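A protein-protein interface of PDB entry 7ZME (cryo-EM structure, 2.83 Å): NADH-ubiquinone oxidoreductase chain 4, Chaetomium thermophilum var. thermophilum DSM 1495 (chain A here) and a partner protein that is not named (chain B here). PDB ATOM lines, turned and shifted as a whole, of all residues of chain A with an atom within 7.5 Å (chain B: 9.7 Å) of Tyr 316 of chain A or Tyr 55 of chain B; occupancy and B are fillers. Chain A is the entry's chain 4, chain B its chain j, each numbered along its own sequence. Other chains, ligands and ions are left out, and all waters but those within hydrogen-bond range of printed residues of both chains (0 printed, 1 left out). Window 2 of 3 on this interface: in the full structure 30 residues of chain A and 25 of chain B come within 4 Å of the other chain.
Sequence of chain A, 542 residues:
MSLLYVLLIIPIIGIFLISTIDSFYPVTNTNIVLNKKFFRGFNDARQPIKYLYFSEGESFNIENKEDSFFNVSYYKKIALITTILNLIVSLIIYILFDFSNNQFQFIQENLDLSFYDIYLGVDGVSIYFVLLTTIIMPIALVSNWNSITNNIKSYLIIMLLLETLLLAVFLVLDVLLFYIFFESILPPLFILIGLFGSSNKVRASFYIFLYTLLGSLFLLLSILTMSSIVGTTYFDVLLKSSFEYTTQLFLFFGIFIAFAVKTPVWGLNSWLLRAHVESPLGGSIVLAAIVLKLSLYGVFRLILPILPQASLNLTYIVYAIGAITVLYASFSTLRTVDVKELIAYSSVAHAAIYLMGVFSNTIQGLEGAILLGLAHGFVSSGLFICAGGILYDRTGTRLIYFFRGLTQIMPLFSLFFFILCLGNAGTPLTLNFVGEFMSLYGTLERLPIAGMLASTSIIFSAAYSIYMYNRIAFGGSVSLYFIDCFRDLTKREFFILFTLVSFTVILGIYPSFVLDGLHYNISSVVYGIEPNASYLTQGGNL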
ATOM      1  N   ALA A 310       3.019 -20.548 -32.317  1.00  0.00           N
ATOM      2  CA  ALA A 310       2.604 -21.712 -33.136  1.00  0.00           C
ATOM      3  C   ALA A 310       2.428 -22.910 -32.220  1.00  0.00           C
ATOM      4  O   ALA A 310       1.456 -23.640 -32.374  1.00  0.00           O
ATOM      5  CB  ALA A 310       3.633 -22.005 -34.192  1.00  0.00           C
ATOM      6  N   SER A 311       3.362 -23.086 -31.293  1.00  0.00           N
ATOM      7  CA  SER A 311       3.266 -24.223 -30.352  1.00  0.00           C
ATOM      8  C   SER A 311       1.972 -24.080 -29.574  1.00  0.00           C
ATOM      9  O   SER A 311       1.253 -25.074 -29.482  1.00  0.00           O
ATOM     10  CB  SER A 311       4.434 -24.240 -29.418  1.00  0.00           C
ATOM     11  OG  SER A 311       4.226 -25.186 -28.387  1.00  0.00           O
ATOM     12  N   LEU A 312       1.669 -22.877 -29.092  1.00  0.00           N
ATOM     13  CA  LEU A 312       0.451 -22.673 -28.274  1.00  0.00           C
ATOM     14  C   LEU A 312      -0.790 -22.976 -29.118  1.00  0.00           C
ATOM     15  O   LEU A 312      -1.670 -23.696 -28.624  1.00  0.00           O
ATOM     16  CB  LEU A 312       0.444 -21.223 -27.787  1.00  0.00           C
ATOM     17  CG  LEU A 312      -0.577 -20.896 -26.700  1.00  0.00           C
ATOM     18  CD1 LEU A 312      -0.267 -21.655 -25.421  1.00  0.00           C
ATOM     19  CD2 LEU A 312      -0.613 -19.402 -26.432  1.00  0.00           C
ATOM     20  N   ASN A 313      -0.845 -22.463 -30.345  1.00  0.00           N
ATOM     21  CA  ASN A 313      -2.024 -22.642 -31.231  1.00  0.00           C
ATOM     22  C   ASN A 313      -2.168 -24.073 -31.752  1.00  0.00           C
ATOM     23  O   ASN A 313      -3.313 -24.519 -31.893  1.00  0.00           O
ATOM     24  CB  ASN A 313      -2.137 -21.530 -32.269  1.00  0.00           C
ATOM     25  CG  ASN A 313      -2.571 -20.215 -31.655  1.00  0.00           C
ATOM     26  OD1 ASN A 313      -2.173 -19.880 -30.545  1.00  0.00           O
ATOM     27  ND2 ASN A 313      -3.389 -19.461 -32.370  1.00  0.00           N
ATOM     28  N   LEU A 314      -1.068 -24.763 -32.034  1.00  0.00           N
ATOM     29  CA  LEU A 314      -1.146 -26.107 -32.662  1.00  0.00           C
ATOM     30  C   LEU A 314      -1.064 -27.216 -31.614  1.00  0.00           C
ATOM     31  O   LEU A 314      -0.905 -28.375 -32.009  1.00  0.00           O
ATOM     32  CB  LEU A 314      -0.038 -26.225 -33.710  1.00  0.00           C
ATOM     33  CG  LEU A 314      -0.061 -25.142 -34.783  1.00  0.00           C
ATOM     34  CD1 LEU A 314       1.139 -25.269 -35.696  1.00  0.00           C
ATOM     35  CD2 LEU A 314      -1.355 -25.188 -35.579  1.00  0.00           C
ATOM     36  N   THR A 315      -1.190 -26.873 -30.334  1.00  0.00           N
ATOM     37  CA  THR A 315      -1.085 -27.868 -29.234  1.00  0.00           C
ATOM     38  C   THR A 315      -2.182 -28.928 -29.385  1.00  0.00           C
ATOM     39  O   THR A 315      -1.914 -30.083 -29.054  1.00  0.00           O
ATOM     40  CB  THR A 315      -1.015 -27.196 -27.853  1.00  0.00           C
ATOM     41  OG1 THR A 315       0.237 -26.526 -27.726  1.00  0.00           O
ATOM     42  CG2 THR A 315      -1.145 -28.168 -26.702  1.00  0.00           C
ATOM     43  N   TYR A 316      -3.335 -28.570 -29.942  1.00  0.00           N
ATOM     44  CA  TYR A 316      -4.463 -29.530 -29.999  1.00  0.00           C
ATOM     45  C   TYR A 316      -4.160 -30.571 -31.074  1.00  0.00           C
ATOM     46  O   TYR A 316      -4.646 -31.701 -30.933  1.00  0.00           O
ATOM     47  CB  TYR A 316      -5.779 -28.788 -30.239  1.00  0.00           C
ATOM     48  CG  TYR A 316      -5.982 -28.259 -31.635  1.00  0.00           C
ATOM     49  CD1 TYR A 316      -5.460 -27.036 -32.018  1.00  0.00           C
ATOM     50  CD2 TYR A 316      -6.707 -28.977 -32.570  1.00  0.00           C
ATOM     51  CE1 TYR A 316      -5.645 -26.541 -33.296  1.00  0.00           C
ATOM     52  CE2 TYR A 316      -6.897 -28.499 -33.855  1.00  0.00           C
ATOM     53  CZ  TYR A 316      -6.366 -27.276 -34.218  1.00  0.00           C
ATOM     54  OH  TYR A 316      -6.552 -26.797 -35.481  1.00  0.00           O
ATOM     55  N   ILE A 317      -3.404 -30.206 -32.113  1.00  0.00           N
ATOM     56  CA  ILE A 317      -2.969 -31.218 -33.072  1.00  0.00           C
ATOM     57  C   ILE A 317      -2.001 -32.181 -32.405  1.00  0.00           C
ATOM     58  O   ILE A 317      -2.133 -33.404 -32.516  1.00  0.00           O
ATOM     59  CB  ILE A 317      -2.329 -30.581 -34.318  1.00  0.00           C
ATOM     60  CG1 ILE A 317      -3.304 -29.680 -35.066  1.00  0.00           C
ATOM     61  CG2 ILE A 317      -1.804 -31.651 -35.254  1.00  0.00           C
ATOM     62  CD1 ILE A 317      -3.152 -28.251 -34.721  1.00  0.00           C
ATOM     63  N   VAL A 318      -1.010 -31.636 -31.702  1.00  0.00           N
ATOM     64  CA  VAL A 318       0.002 -32.462 -31.055  1.00  0.00           C
ATOM     65  C   VAL A 318      -0.640 -33.372 -30.020  1.00  0.00           C
ATOM     66  O   VAL A 318      -0.310 -34.558 -29.922  1.00  0.00           O
ATOM     67  CB  VAL A 318       1.087 -31.564 -30.432  1.00  0.00           C
ATOM     68  CG1 VAL A 318       2.075 -32.389 -29.621  1.00  0.00           C
ATOM     69  CG2 VAL A 318       1.794 -30.777 -31.511  1.00  0.00           C
ATOM     70  N   TYR A 319      -1.575 -32.834 -29.240  1.00  0.00           N
ATOM     71  CA  TYR A 319      -2.208 -33.627 -28.197  1.00  0.00           C
ATOM     72  C   TYR A 319      -3.173 -34.648 -28.782  1.00  0.00           C
ATOM     73  O   TYR A 319      -3.414 -35.692 -28.168  1.00  0.00           O
ATOM     74  CB  TYR A 319      -2.908 -32.704 -27.202  1.00  0.00           C
ATOM     75  CG  TYR A 319      -1.973 -32.168 -26.141  1.00  0.00           C
ATOM     76  CD1 TYR A 319      -0.598 -32.234 -26.308  1.00  0.00           C
ATOM     77  CD2 TYR A 319      -2.460 -31.605 -24.974  1.00  0.00           C
ATOM     78  CE1 TYR A 319       0.259 -31.749 -25.351  1.00  0.00           C
ATOM     79  CE2 TYR A 319      -1.610 -31.117 -24.010  1.00  0.00           C
ATOM     80  CZ  TYR A 319      -0.251 -31.193 -24.203  1.00  0.00           C
ATOM     81  OH  TYR A 319       0.604 -30.717 -23.245  1.00  0.00           O
ATOM     82  N   ALA A 320      -3.727 -34.373 -29.961  1.00  0.00           N
ATOM     83  CA  ALA A 320      -4.526 -35.379 -30.650  1.00  0.00           C
ATOM     84  C   ALA A 320      -3.654 -36.534 -31.117  1.00  0.00           C
ATOM     85  O   ALA A 320      -3.983 -37.703 -30.893  1.00  0.00           O
ATOM     86  CB  ALA A 320      -5.262 -34.749 -31.830  1.00  0.00           C
ATOM     87  N   ILE A 321      -2.532 -36.223 -31.765  1.00  0.00           N
ATOM     88  CA  ILE A 321      -1.606 -37.265 -32.194  1.00  0.00           C
ATOM     89  C   ILE A 321      -1.051 -38.013 -30.992  1.00  0.00           C
ATOM     90  O   ILE A 321      -0.964 -39.246 -30.997  1.00  0.00           O
ATOM     91  CB  ILE A 321      -0.484 -36.654 -33.053  1.00  0.00           C
ATOM     92  CG1 ILE A 321      -1.067 -36.008 -34.309  1.00  0.00           C
ATOM     93  CG2 ILE A 321       0.543 -37.703 -33.421  1.00  0.00           C
ATOM     94  CD1 ILE A 321      -0.236 -34.871 -34.849  1.00  0.00           C
ATOM     95  N   GLY A 322      -0.677 -37.282 -29.939  1.00  0.00           N
ATOM     96  CA  GLY A 322      -0.096 -37.922 -28.772  1.00  0.00           C
ATOM     97  C   GLY A 322      -1.058 -38.853 -28.061  1.00  0.00           C
ATOM     98  O   GLY A 322      -0.684 -39.955 -27.655  1.00  0.00           O
ATOM     99  N   ARG A 446      -2.730 -28.336 -19.263  1.00  0.00           N
ATOM    100  CA  ARG A 446      -2.753 -27.617 -20.531  1.00  0.00           C
ATOM    101  C   ARG A 446      -4.032 -27.910 -21.311  1.00  0.00           C
ATOM    102  O   ARG A 446      -4.764 -26.988 -21.686  1.00  0.00           O
ATOM    103  CB  ARG A 446      -1.511 -27.980 -21.349  1.00  0.00           C
ATOM    104  CG  ARG A 446      -1.545 -27.534 -22.792  1.00  0.00           C
ATOM    105  CD  ARG A 446      -1.118 -26.088 -22.931  1.00  0.00           C
ATOM    106  NE  ARG A 446      -1.520 -25.502 -24.207  1.00  0.00           N
ATOM    107  CZ  ARG A 446      -2.771 -25.203 -24.539  1.00  0.00           C
ATOM    108  NH1 ARG A 446      -3.033 -24.674 -25.721  1.00  0.00           N
ATOM    109  NH2 ARG A 446      -3.763 -25.423 -23.689  1.00  0.00           N
ATOM    110  N   LEU A 447      -4.307 -29.184 -21.577  1.00  0.00           N
ATOM    111  CA  LEU A 447      -5.583 -29.618 -22.143  1.00  0.00           C
ATOM    112  C   LEU A 447      -6.120 -30.755 -21.290  1.00  0.00           C
ATOM    113  O   LEU A 447      -5.640 -31.895 -21.394  1.00  0.00           O
ATOM    114  CB  LEU A 447      -5.464 -30.047 -23.603  1.00  0.00           C
ATOM    115  CG  LEU A 447      -5.206 -28.932 -24.607  1.00  0.00           C
ATOM    116  CD1 LEU A 447      -4.936 -29.467 -25.993  1.00  0.00           C
ATOM    117  CD2 LEU A 447      -6.433 -28.066 -24.625  1.00  0.00           C
ATOM    118  N   ILE A 449      -8.826 -32.733 -21.365  1.00  0.00           N
ATOM    119  CA  ILE A 449      -9.317 -33.952 -22.000  1.00  0.00           C
ATOM    120  C   ILE A 449      -8.180 -34.734 -22.650  1.00  0.00           C
ATOM    121  O   ILE A 449      -8.206 -35.969 -22.669  1.00  0.00           O
ATOM    122  CB  ILE A 449     -10.435 -33.628 -23.006  1.00  0.00           C
ATOM    123  CG1 ILE A 449      -9.870 -32.945 -24.247  1.00  0.00           C
ATOM    124  CG2 ILE A 449     -11.497 -32.757 -22.354  1.00  0.00           C
ATOM    125  CD1 ILE A 449     -10.760 -33.068 -25.427  1.00  0.00           C
ATOM    126  N   ALA A 450      -7.177 -34.047 -23.198  1.00  0.00           N
ATOM    127  CA  ALA A 450      -6.023 -34.750 -23.748  1.00  0.00           C
ATOM    128  C   ALA A 450      -5.189 -35.382 -22.642  1.00  0.00           C
ATOM    129  O   ALA A 450      -4.690 -36.501 -22.797  1.00  0.00           O
ATOM    130  CB  ALA A 450      -5.176 -33.793 -24.583  1.00  0.00           C
ATOM    131  N   VAL B  46     -11.326 -41.106 -35.526  1.00  0.00           N
ATOM    132  CA  VAL B  46     -10.987 -41.063 -34.103  1.00  0.00           C
ATOM    133  C   VAL B  46      -9.993 -39.953 -33.786  1.00  0.00           C
ATOM    134  O   VAL B  46     -10.221 -39.210 -32.818  1.00  0.00           O
ATOM    135  CB  VAL B  46     -10.516 -42.450 -33.626  1.00  0.00           C
ATOM    136  CG1 VAL B  46     -10.128 -42.401 -32.167  1.00  0.00           C
ATOM    137  CG2 VAL B  46     -11.603 -43.482 -33.842  1.00  0.00           C
ATOM    138  N   PRO B  47      -8.885 -39.785 -34.522  1.00  0.00           N
ATOM    139  CA  PRO B  47      -8.044 -38.603 -34.275  1.00  0.00           C
ATOM    140  C   PRO B  47      -8.764 -37.288 -34.502  1.00  0.00           C
ATOM    141  O   PRO B  47      -8.541 -36.329 -33.756  1.00  0.00           O
ATOM    142  CB  PRO B  47      -6.885 -38.796 -35.261  1.00  0.00           C
ATOM    143  CG  PRO B  47      -6.815 -40.251 -35.458  1.00  0.00           C
ATOM    144  CD  PRO B  47      -8.229 -40.717 -35.456  1.00  0.00           C
ATOM    145  N   SER B  48      -9.628 -37.213 -35.514  1.00  0.00           N
ATOM    146  CA  SER B  48     -10.348 -35.974 -35.782  1.00  0.00           C
ATOM    147  C   SER B  48     -11.276 -35.621 -34.629  1.00  0.00           C
ATOM    148  O   SER B  48     -11.352 -34.461 -34.213  1.00  0.00           O
ATOM    149  CB  SER B  48     -11.132 -36.094 -37.085  1.00  0.00           C
ATOM    150  OG  SER B  48     -10.260 -36.312 -38.178  1.00  0.00           O
ATOM    151  N   THR B  49     -11.996 -36.613 -34.105  1.00  0.00           N
ATOM    152  CA  THR B  49     -12.871 -36.381 -32.963  1.00  0.00           C
ATOM    153  C   THR B  49     -12.077 -35.937 -31.743  1.00  0.00           C
ATOM    154  O   THR B  49     -12.438 -34.970 -31.066  1.00  0.00           O
ATOM    155  CB  THR B  49     -13.667 -37.650 -32.656  1.00  0.00           C
ATOM    156  OG1 THR B  49     -14.245 -38.155 -33.864  1.00  0.00           O
ATOM    157  CG2 THR B  49     -14.772 -37.354 -31.655  1.00  0.00           C
ATOM    158  N   ILE B  50     -10.980 -36.638 -31.449  1.00  0.00           N
ATOM    159  CA  ILE B  50     -10.162 -36.284 -30.294  1.00  0.00           C
ATOM    160  C   ILE B  50      -9.564 -34.895 -30.472  1.00  0.00           C
ATOM    161  O   ILE B  50      -9.535 -34.091 -29.533  1.00  0.00           O
ATOM    162  CB  ILE B  50      -9.074 -37.351 -30.063  1.00  0.00           C
ATOM    163  CG1 ILE B  50      -9.683 -38.589 -29.408  1.00  0.00           C
ATOM    164  CG2 ILE B  50      -7.939 -36.799 -29.216  1.00  0.00           C
ATOM    165  CD1 ILE B  50      -8.736 -39.748 -29.307  1.00  0.00           C
ATOM    166  N   GLY B  51      -9.081 -34.592 -31.676  1.00  0.00           N
ATOM    167  CA  GLY B  51      -8.518 -33.276 -31.929  1.00  0.00           C
ATOM    168  C   GLY B  51      -9.549 -32.167 -31.867  1.00  0.00           C
ATOM    169  O   GLY B  51      -9.265 -31.072 -31.375  1.00  0.00           O
ATOM    170  N   TYR B  52     -10.756 -32.425 -32.374  1.00  0.00           N
ATOM    171  CA  TYR B  52     -11.791 -31.398 -32.366  1.00  0.00           C
ATOM    172  C   TYR B  52     -12.218 -31.049 -30.944  1.00  0.00           C
ATOM    173  O   TYR B  52     -12.402 -29.871 -30.616  1.00  0.00           O
ATOM    174  CB  TYR B  52     -12.989 -31.856 -33.199  1.00  0.00           C
ATOM    175  CG  TYR B  52     -14.232 -31.010 -33.030  1.00  0.00           C
ATOM    176  CD1 TYR B  52     -15.164 -31.290 -32.042  1.00  0.00           C
ATOM    177  CD2 TYR B  52     -14.469 -29.926 -33.860  1.00  0.00           C
ATOM    178  CE1 TYR B  52     -16.289 -30.523 -31.887  1.00  0.00           C
ATOM    179  CE2 TYR B  52     -15.593 -29.152 -33.711  1.00  0.00           C
ATOM    180  CZ  TYR B  52     -16.501 -29.454 -32.725  1.00  0.00           C
ATOM    181  OH  TYR B  52     -17.629 -28.683 -32.571  1.00  0.00           O
ATOM    182  N   LEU B  53     -12.390 -32.055 -30.085  1.00  0.00           N
ATOM    183  CA  LEU B  53     -12.766 -31.776 -28.704  1.00  0.00           C
ATOM    184  C   LEU B  53     -11.651 -31.054 -27.960  1.00  0.00           C
ATOM    185  O   LEU B  53     -11.921 -30.242 -27.068  1.00  0.00           O
ATOM    186  CB  LEU B  53     -13.158 -33.065 -27.981  1.00  0.00           C
ATOM    187  CG  LEU B  53     -14.585 -33.603 -28.138  1.00  0.00           C
ATOM    188  CD1 LEU B  53     -15.574 -32.615 -27.544  1.00  0.00           C
ATOM    189  CD2 LEU B  53     -14.951 -33.918 -29.577  1.00  0.00           C
ATOM    190  N   ALA B  54     -10.395 -31.342 -28.299  1.00  0.00           N
ATOM    191  CA  ALA B  54      -9.288 -30.585 -27.726  1.00  0.00           C
ATOM    192  C   ALA B  54      -9.339 -29.127 -28.162  1.00  0.00           C
ATOM    193  O   ALA B  54      -9.053 -28.222 -27.372  1.00  0.00           O
ATOM    194  CB  ALA B  54      -7.958 -31.221 -28.121  1.00  0.00           C
ATOM    195  N   TYR B  55      -9.698 -28.883 -29.426  1.00  0.00           N
ATOM    196  CA  TYR B  55      -9.838 -27.517 -29.916  1.00  0.00           C
ATOM    197  C   TYR B  55     -10.949 -26.773 -29.188  1.00  0.00           C
ATOM    198  O   TYR B  55     -10.799 -25.593 -28.851  1.00  0.00           O
ATOM    199  CB  TYR B  55     -10.098 -27.533 -31.422  1.00  0.00           C
ATOM    200  CG  TYR B  55     -10.005 -26.175 -32.077  1.00  0.00           C
ATOM    201  CD1 TYR B  55      -8.796 -25.696 -32.550  1.00  0.00           C
ATOM    202  CD2 TYR B  55     -11.131 -25.376 -32.226  1.00  0.00           C
ATOM    203  CE1 TYR B  55      -8.705 -24.460 -33.149  1.00  0.00           C
ATOM    204  CE2 TYR B  55     -11.050 -24.136 -32.824  1.00  0.00           C
ATOM    205  CZ  TYR B  55      -9.834 -23.682 -33.285  1.00  0.00           C
ATOM    206  OH  TYR B  55      -9.746 -22.446 -33.884  1.00  0.00           O
ATOM    207  N   LYS B  56     -12.073 -27.440 -28.939  1.00  0.00           N
ATOM    208  CA  LYS B  56     -13.235 -26.790 -28.343  1.00  0.00           C
ATOM    209  C   LYS B  56     -13.160 -26.691 -26.828  1.00  0.00           C
ATOM    210  O   LYS B  56     -14.067 -26.121 -26.218  1.00  0.00           O
ATOM    211  CB  LYS B  56     -14.513 -27.530 -28.740  1.00  0.00           C
ATOM    212  CG  LYS B  56     -14.779 -27.552 -30.230  1.00  0.00           C
ATOM    213  CD  LYS B  56     -14.962 -26.148 -30.775  1.00  0.00           C
ATOM    214  CE  LYS B  56     -16.228 -25.508 -30.233  1.00  0.00           C
ATOM    215  NZ  LYS B  56     -17.449 -26.224 -30.695  1.00  0.00           N
ATOM    216  N   THR B  57     -12.113 -27.227 -26.207  1.00  0.00           N
ATOM    217  CA  THR B  57     -11.948 -27.140 -24.764  1.00  0.00           C
ATOM    218  C   THR B  57     -10.632 -26.486 -24.370  1.00  0.00           C
ATOM    219  O   THR B  57     -10.212 -26.615 -23.215  1.00  0.00           O
ATOM    220  CB  THR B  57     -12.043 -28.531 -24.123  1.00  0.00           C
ATOM    221  OG1 THR B  57     -11.071 -29.399 -24.712  1.00  0.00           O
ATOM    222  CG2 THR B  57     -13.425 -29.120 -24.331  1.00  0.00           C
ATOM    223  N   ASP B  58      -9.973 -25.786 -25.284  1.00  0.00           N
ATOM    224  CA  ASP B  58      -8.651 -25.238 -25.014  1.00  0.00           C
ATOM    225  C   ASP B  58      -8.788 -23.857 -24.382  1.00  0.00           C
ATOM    226  O   ASP B  58      -9.309 -22.928 -25.007  1.00  0.00           O
ATOM    227  CB  ASP B  58      -7.833 -25.177 -26.299  1.00  0.00           C
ATOM    228  CG  ASP B  58      -6.373 -24.919 -26.039  1.00  0.00           C
ATOM    229  OD1 ASP B  58      -5.993 -24.814 -24.857  1.00  0.00           O
ATOM    230  OD2 ASP B  58      -5.599 -24.834 -27.014  1.00  0.00           O
ATOM    231  N   GLY B  59      -8.313 -23.725 -23.147  1.00  0.00           N
ATOM    232  CA  GLY B  59      -8.527 -22.531 -22.366  1.00  0.00           C
ATOM    233  C   GLY B  59      -9.862 -22.471 -21.662  1.00  0.00           C
ATOM    234  O   GLY B  59     -10.150 -21.468 -21.002  1.00  0.00           O
ATOM    235  N   LEU B  60     -10.684 -23.514 -21.779  1.00  0.00           N
ATOM    236  CA  LEU B  60     -12.033 -23.474 -21.230  1.00  0.00           C
ATOM    237  C   LEU B  60     -12.024 -23.471 -19.708  1.00  0.00           C
ATOM    238  O   LEU B  60     -12.826 -22.772 -19.082  1.00  0.00           O
ATOM    239  CB  LEU B  60     -12.842 -24.657 -21.757  1.00  0.00           C
ATOM    240  CG  LEU B  60     -14.319 -24.759 -21.380  1.00  0.00           C
ATOM    241  CD1 LEU B  60     -15.032 -23.428 -21.563  1.00  0.00           C
ATOM    242  CD2 LEU B  60     -14.976 -25.839 -22.209  1.00  0.00           C
ATOM    243  N   ARG B  75     -13.786 -19.376 -20.361  1.00  0.00           N
ATOM    244  CA  ARG B  75     -14.258 -18.994 -21.682  1.00  0.00           C
ATOM    245  C   ARG B  75     -15.780 -19.057 -21.730  1.00  0.00           C
ATOM    246  O   ARG B  75     -16.392 -19.839 -21.004  1.00  0.00           O
ATOM    247  CB  ARG B  75     -13.644 -19.904 -22.747  1.00  0.00           C
ATOM    248  CG  ARG B  75     -14.099 -19.609 -24.164  1.00  0.00           C
ATOM    249  CD  ARG B  75     -13.038 -20.003 -25.173  1.00  0.00           C
ATOM    250  NE  ARG B  75     -12.358 -21.250 -24.829  1.00  0.00           N
ATOM    251  CZ  ARG B  75     -12.883 -22.463 -24.977  1.00  0.00           C
ATOM    252  NH1 ARG B  75     -12.181 -23.532 -24.641  1.00  0.00           N
ATOM    253  NH2 ARG B  75     -14.100 -22.611 -25.482  1.00  0.00           N
ATOM    254  OXT ARG B  75     -16.435 -18.333 -22.482  1.00  0.00           O
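Tyr 316 of chain A touches just these residues of chain B: Gly 51 (3.5 Å), Ala 54 (3.9 Å) and Tyr 55 (3.3 Å). No residue of chain B comes within 4 Å of Ile 317 of chain A. Of the printed residues of chain B, Ala 320 of chain A touches Ile 50 (3.97 Å) and Gly 51 (3.6 Å). Gly 322 of chain A touches none of the printed residues of chain B. Of the printed residues of chain B, Arg 446 of chain A touches Asp 58 (2.6 Å). Thr 49 of chain B touches none of the printed residues of chain A. Of the printed residues of chain A, Leu 53 of chain B touches Ile 449 (3.4 Å). Of chain A, only Tyr 316 (3.9 Å), Leu 447 (3.8 Å) and Ile 449 (3.4 Å) come within 4 Å of Ala 54 of chain B. Tyr 55 of chain B touches just one residue of chain A: Tyr 316. The nearest residue of chain A that does not touch Tyr 55 of chain B is Asn 313 of chain A (5.5 Å). The nearest printed residue of chain B that does not touch Leu 447 of chain A is Thr 57 of chain B (4.3 Å).
CD2 of Tyr 316 of chain A touches O of Gly 51 of chain B, 3.5 Å away. CB of Tyr 316 of chain A touches CB of Ala 54 of chain B (3.9 Å). Tyr 316 of chain A touches Tyr 55 of chain B. Ala 320 of chain A touches Ile 50 of chain B. Gly 51 of chain B touches Ala 320 of chain A (CA to CB, 3.6 Å). Ala 54 of chain B touches Leu 447 of chain A. CD2 of Leu 447 of chain A touches OD1 of Asp 58 of chain B (3.3 Å). CD1 of Ile 449 of chain A touches C of Leu 53 of chain B (3.4 Å). CD1 of Ile 449 of chain A touches N of Ala 54 of chain B, 3.4 Å away. Ile 449 of chain A touches Thr 57 of chain B.
The side-chain carboxylate (OD1) of Asp 58 of chain B is in salt-bridge range of the guanidinium group (NH2) of Arg 446 of chain A (2.6 Å).
The backbone carbonyl oxygen (O) of Leu 53 of chain B sits at hydrogen-bond distance from the side-chain hydroxyl (OG1) of Thr 57 of chain B, at 2.6 Å. The backbone carbonyl oxygen (O) of Asp 58 of chain B sits at hydrogen-bond distance from the guanidinium group (NH1) of Arg 75 of chain B (3.0 Å). The backbone carbonyl oxygen (O) of Leu 312 of chain A lies within hydrogen-bond range of the guanidinium group (NH1) of Arg 446 of chain A.
Of the 17 printed residues of chain A, 5 touch a printed residue of chain B. Printed residues of chain A that touch a printed residue of chain B: Tyr 316, Ala 320, Arg 446, Leu 447 and Ile 449. Among the printed residues, 11 pairs touch across the chains.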
